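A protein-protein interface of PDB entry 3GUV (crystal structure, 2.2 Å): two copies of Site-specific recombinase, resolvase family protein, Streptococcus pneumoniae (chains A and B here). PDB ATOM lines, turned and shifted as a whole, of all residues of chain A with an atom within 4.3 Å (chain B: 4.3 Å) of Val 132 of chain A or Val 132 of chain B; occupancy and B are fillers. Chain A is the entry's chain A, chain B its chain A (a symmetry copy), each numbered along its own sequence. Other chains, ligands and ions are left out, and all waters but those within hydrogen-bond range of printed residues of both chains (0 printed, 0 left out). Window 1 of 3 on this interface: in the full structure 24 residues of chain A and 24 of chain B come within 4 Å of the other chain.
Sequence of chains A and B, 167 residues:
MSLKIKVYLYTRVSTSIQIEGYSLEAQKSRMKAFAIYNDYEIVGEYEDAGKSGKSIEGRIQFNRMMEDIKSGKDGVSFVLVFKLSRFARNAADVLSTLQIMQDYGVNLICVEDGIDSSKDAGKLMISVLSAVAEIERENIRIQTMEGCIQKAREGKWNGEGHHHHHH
Ala 91 of chain A touches Val 132 of chain B, and with the chains exchanged Val 132 of chain A touches Ala 91 of chain B.
Leu 129 of chain A touches Val 132 of chain B, and with the chains exchanged Val 132 of chain A touches Leu 129 of chain B.
Val 132 of chain A touches its own counterpart, Val 132 of chain B.
Positions printed for both chains: 91, 128, 129, 130, 131, 132, 133, 134, 135 and 136.
Of the 5 pairs that touch across the chains among the printed residues, 5 have their exchanged pair printed and touching as well.
Printed residues of chain A that touch a printed residue of chain B: Ala 91, Leu 129 and Val 132.
Of the 10 printed residues of chain B, 3 touch a printed residue of chain A.
Hydrophobic or aromatic side chains of chain B within 4 Å of the printed part of chain A: Ala 91, Leu 129 and Val 132.
Among the printed residues, 5 pairs touch across the chains.
Among the printed residues, merely in contact across the chains: Ala 91 of chain A with Val 132 of chain B (3.9 Å), Leu 129 of chain A with Val 132 of chain B (3.8 Å), Val 132 of chain A with Ala 91 of chain B (3.9 Å), Val 132 of chain A with Leu 129 of chain B (3.8 Å) and Val 132 of chain A with Val 132 of chain B (3.9 Å).
Of the printed residues of chain B, Ala 91 of chain A touches Val 132.
Of the printed residues of chain B, Leu 129 of chain A touches Val 132.
Of chain B, only Ala 91 (3.9 Å), Leu 129 (3.8 Å) and Val 132 (3.9 Å) come within 4 Å of Val 132 of chain A.
Of the printed residues of chain A, Ala 91 of chain B touches Val 132 (3.9 Å).
Of chain A, only Ala 91 (3.9 Å), Leu 129 (3.8 Å) and Val 132 (3.9 Å) come within 4 Å of Val 132 of chain B.
The nearest printed residue of chain B that does not touch Val 132 of chain A is Glu 136 of chain B (4.9 Å).
The nearest printed residue of chain B that does not touch Leu 129 of chain A is Val 128 of chain B (4.1 Å).
The backbone NH of Ala 91 of chain A lies within hydrogen-bond range of the side-chain carboxylate of Glu 136 of chain A (2.8 Å).
The backbone NH of Ala 91 of chain B is in hydrogen-bond range of the side-chain carboxylate of Glu 136 of chain B (2.8 Å).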
ATOM      1  N   ALA A  91       2.179  17.407  -8.765  1.00  0.00           N
ATOM      2  CA  ALA A  91       2.266  16.456  -7.664  1.00  0.00           C
ATOM      3  C   ALA A  91       0.972  16.395  -6.839  1.00  0.00           C
ATOM      4  O   ALA A  91       0.578  15.301  -6.365  1.00  0.00           O
ATOM      5  CB  ALA A  91       3.485  16.802  -6.754  1.00  0.00           C
ATOM      6  N   VAL A 128       6.060  11.132  -0.031  1.00  0.00           N
ATOM      7  CA  VAL A 128       6.904  11.927  -0.901  1.00  0.00           C
ATOM      8  C   VAL A 128       6.012  12.878  -1.674  1.00  0.00           C
ATOM      9  O   VAL A 128       6.256  14.088  -1.726  1.00  0.00           O
ATOM     10  CB  VAL A 128       7.748  11.028  -1.848  1.00  0.00           C
ATOM     11  CG1 VAL A 128       8.516  11.863  -2.838  1.00  0.00           C
ATOM     12  CG2 VAL A 128       8.713  10.153  -1.027  1.00  0.00           C
ATOM     13  N   LEU A 129       4.956  12.329  -2.258  1.00  0.00           N
ATOM     14  CA  LEU A 129       4.051  13.104  -3.118  1.00  0.00           C
ATOM     15  C   LEU A 129       3.409  14.263  -2.317  1.00  0.00           C
ATOM     16  O   LEU A 129       3.337  15.423  -2.773  1.00  0.00           O
ATOM     17  CB  LEU A 129       2.953  12.190  -3.720  1.00  0.00           C
ATOM     18  CG  LEU A 129       3.175  11.394  -5.026  1.00  0.00           C
ATOM     19  CD1 LEU A 129       1.979  10.474  -5.277  1.00  0.00           C
ATOM     20  CD2 LEU A 129       3.435  12.286  -6.242  1.00  0.00           C
ATOM     21  N   SER A 130       2.929  13.917  -1.127  1.00  0.00           N
ATOM     22  CA  SER A 130       2.400  14.890  -0.205  1.00  0.00           C
ATOM     23  C   SER A 130       3.453  15.974   0.103  1.00  0.00           C
ATOM     24  O   SER A 130       3.141  17.164   0.040  1.00  0.00           O
ATOM     25  CB  SER A 130       1.928  14.204   1.084  1.00  0.00           C
ATOM     26  OG  SER A 130       1.426  15.205   1.931  1.00  0.00           O
ATOM     27  N   ALA A 131       4.705  15.555   0.338  1.00  0.00           N
ATOM     28  CA  ALA A 131       5.811  16.492   0.650  1.00  0.00           C
ATOM     29  C   ALA A 131       6.109  17.407  -0.523  1.00  0.00           C
ATOM     30  O   ALA A 131       6.417  18.592  -0.309  1.00  0.00           O
ATOM     31  CB  ALA A 131       7.079  15.726   1.083  1.00  0.00           C
ATOM     32  N   VAL A 132       5.990  16.885  -1.761  1.00  0.00           N
ATOM     33  CA  VAL A 132       6.288  17.676  -2.952  1.00  0.00           C
ATOM     34  C   VAL A 132       5.109  18.552  -3.270  1.00  0.00           C
ATOM     35  O   VAL A 132       5.293  19.651  -3.803  1.00  0.00           O
ATOM     36  CB  VAL A 132       6.670  16.817  -4.203  1.00  0.00           C
ATOM     37  CG1 VAL A 132       6.786  17.702  -5.471  1.00  0.00           C
ATOM     38  CG2 VAL A 132       7.958  16.028  -3.957  1.00  0.00           C
ATOM     39  N   ALA A 133       3.900  18.076  -2.977  1.00  0.00           N
ATOM     40  CA  ALA A 133       2.682  18.905  -3.126  1.00  0.00           C
ATOM     41  C   ALA A 133       2.759  20.125  -2.202  1.00  0.00           C
ATOM     42  O   ALA A 133       2.355  21.229  -2.595  1.00  0.00           O
ATOM     43  CB  ALA A 133       1.369  18.073  -2.857  1.00  0.00           C
ATOM     44  N   GLU A 134       3.283  19.926  -0.986  1.00  0.00           N
ATOM     45  CA  GLU A 134       3.567  21.067  -0.036  1.00  0.00           C
ATOM     46  C   GLU A 134       4.573  22.109  -0.628  1.00  0.00           C
ATOM     47  O   GLU A 134       4.372  23.342  -0.504  1.00  0.00           O
ATOM     48  CB  GLU A 134       4.029  20.522   1.312  1.00  0.00           C
ATOM     49  N   ILE A 135       5.605  21.627  -1.335  1.00  0.00           N
ATOM     50  CA  ILE A 135       6.477  22.520  -2.064  1.00  0.00           C
ATOM     51  C   ILE A 135       5.665  23.374  -3.032  1.00  0.00           C
ATOM     52  O   ILE A 135       5.797  24.588  -3.009  1.00  0.00           O
ATOM     53  CB  ILE A 135       7.622  21.819  -2.814  1.00  0.00           C
ATOM     54  CG1 ILE A 135       8.541  21.078  -1.834  1.00  0.00           C
ATOM     55  CG2 ILE A 135       8.424  22.867  -3.623  1.00  0.00           C
ATOM     56  CD1 ILE A 135       9.542  20.089  -2.475  1.00  0.00           C
ATOM     57  N   GLU A 136       4.792  22.765  -3.829  1.00  0.00           N
ATOM     58  CA  GLU A 136       4.031  23.478  -4.874  1.00  0.00           C
ATOM     59  C   GLU A 136       3.068  24.497  -4.276  1.00  0.00           C
ATOM     60  O   GLU A 136       2.921  25.597  -4.816  1.00  0.00           O
ATOM     61  CB  GLU A 136       3.184  22.514  -5.721  1.00  0.00           C
ATOM     62  CG  GLU A 136       3.942  21.330  -6.364  1.00  0.00           C
ATOM     63  CD  GLU A 136       3.018  20.321  -7.084  1.00  0.00           C
ATOM     64  OE1 GLU A 136       1.845  20.089  -6.620  1.00  0.00           O
ATOM     65  OE2 GLU A 136       3.498  19.742  -8.112  1.00  0.00           O
ATOM     66  N   ALA B  91      10.597  19.575  -7.237  1.00  0.00           N
ATOM     67  CA  ALA B  91      10.922  18.155  -7.248  1.00  0.00           C
ATOM     68  C   ALA B  91      12.276  17.870  -7.915  1.00  0.00           C
ATOM     69  O   ALA B  91      13.018  16.960  -7.468  1.00  0.00           O
ATOM     70  CB  ALA B  91       9.783  17.349  -7.948  1.00  0.00           C
ATOM     71  N   VAL B 128       9.790   8.187  -7.858  1.00  0.00           N
ATOM     72  CA  VAL B 128       8.653   9.080  -7.763  1.00  0.00           C
ATOM     73  C   VAL B 128       9.135  10.483  -8.071  1.00  0.00           C
ATOM     74  O   VAL B 128       8.556  11.193  -8.901  1.00  0.00           O
ATOM     75  CB  VAL B 128       7.980   8.994  -6.364  1.00  0.00           C
ATOM     76  CG1 VAL B 128       6.888  10.022  -6.229  1.00  0.00           C
ATOM     77  CG2 VAL B 128       7.413   7.580  -6.134  1.00  0.00           C
ATOM     78  N   LEU B 129      10.217  10.876  -7.416  1.00  0.00           N
ATOM     79  CA  LEU B 129      10.750  12.239  -7.539  1.00  0.00           C
ATOM     80  C   LEU B 129      11.139  12.536  -9.007  1.00  0.00           C
ATOM     81  O   LEU B 129      10.824  13.603  -9.574  1.00  0.00           O
ATOM     82  CB  LEU B 129      11.974  12.435  -6.606  1.00  0.00           C
ATOM     83  CG  LEU B 129      11.817  12.853  -5.127  1.00  0.00           C
ATOM     84  CD1 LEU B 129      13.181  12.812  -4.434  1.00  0.00           C
ATOM     85  CD2 LEU B 129      11.163  14.224  -4.950  1.00  0.00           C
ATOM     86  N   SER B 130      11.846  11.579  -9.599  1.00  0.00           N
ATOM     87  CA  SER B 130      12.195  11.639 -10.996  1.00  0.00           C
ATOM     88  C   SER B 130      10.929  11.778 -11.865  1.00  0.00           C
ATOM     89  O   SER B 130      10.884  12.640 -12.745  1.00  0.00           O
ATOM     90  CB  SER B 130      13.003  10.398 -11.399  1.00  0.00           C
ATOM     91  OG  SER B 130      13.308  10.524 -12.764  1.00  0.00           O
ATOM     92  N   ALA B 131       9.886  10.997 -11.549  1.00  0.00           N
ATOM     93  CA  ALA B 131       8.611  11.029 -12.307  1.00  0.00           C
ATOM     94  C   ALA B 131       7.920  12.372 -12.171  1.00  0.00           C
ATOM     95  O   ALA B 131       7.322  12.852 -13.149  1.00  0.00           O
ATOM     96  CB  ALA B 131       7.675   9.885 -11.862  1.00  0.00           C
ATOM     97  N   VAL B 132       8.020  13.003 -10.982  1.00  0.00           N
ATOM     98  CA  VAL B 132       7.361  14.283 -10.743  1.00  0.00           C
ATOM     99  C   VAL B 132       8.195  15.386 -11.334  1.00  0.00           C
ATOM    100  O   VAL B 132       7.644  16.400 -11.771  1.00  0.00           O
ATOM    101  CB  VAL B 132       7.078  14.578  -9.233  1.00  0.00           C
ATOM    102  CG1 VAL B 132       6.555  16.025  -9.036  1.00  0.00           C
ATOM    103  CG2 VAL B 132       6.105  13.552  -8.645  1.00  0.00           C
ATOM    104  N   ALA B 133       9.517  15.217 -11.331  1.00  0.00           N
ATOM    105  CA  ALA B 133      10.424  16.176 -12.003  1.00  0.00           C
ATOM    106  C   ALA B 133      10.128  16.216 -13.506  1.00  0.00           C
ATOM    107  O   ALA B 133      10.151  17.295 -14.115  1.00  0.00           O
ATOM    108  CB  ALA B 133      11.941  15.836 -11.734  1.00  0.00           C
ATOM    109  N   GLU B 134       9.842  15.048 -14.093  1.00  0.00           N
ATOM    110  CA  GLU B 134       9.374  14.962 -15.528  1.00  0.00           C
ATOM    111  C   GLU B 134       8.048  15.754 -15.779  1.00  0.00           C
ATOM    112  O   GLU B 134       7.910  16.473 -16.799  1.00  0.00           O
ATOM    113  CB  GLU B 134       9.261  13.502 -15.955  1.00  0.00           C
ATOM    114  N   ILE B 135       7.111  15.693 -14.823  1.00  0.00           N
ATOM    115  CA  ILE B 135       5.937  16.535 -14.890  1.00  0.00           C
ATOM    116  C   ILE B 135       6.345  18.002 -14.988  1.00  0.00           C
ATOM    117  O   ILE B 135       5.882  18.689 -15.884  1.00  0.00           O
ATOM    118  CB  ILE B 135       4.949  16.340 -13.728  1.00  0.00           C
ATOM    119  CG1 ILE B 135       4.408  14.904 -13.709  1.00  0.00           C
ATOM    120  CG2 ILE B 135       3.786  17.354 -13.867  1.00  0.00           C
ATOM    121  CD1 ILE B 135       3.651  14.493 -12.425  1.00  0.00           C
ATOM    122  N   GLU B 136       7.244  18.464 -14.123  1.00  0.00           N
ATOM    123  CA  GLU B 136       7.632  19.886 -14.059  1.00  0.00           C
ATOM    124  C   GLU B 136       8.340  20.335 -15.332  1.00  0.00           C
ATOM    125  O   GLU B 136       8.102  21.450 -15.810  1.00  0.00           O
ATOM    126  CB  GLU B 136       8.600  20.162 -12.896  1.00  0.00           C
ATOM    127  CG  GLU B 136       8.128  19.701 -11.498  1.00  0.00           C
ATOM    128  CD  GLU B 136       9.197  19.876 -10.395  1.00  0.00           C
ATOM    129  OE1 GLU B 136      10.438  19.720 -10.681  1.00  0.00           O
ATOM    130  OE2 GLU B 136       8.770  20.149  -9.226  1.00  0.00           O
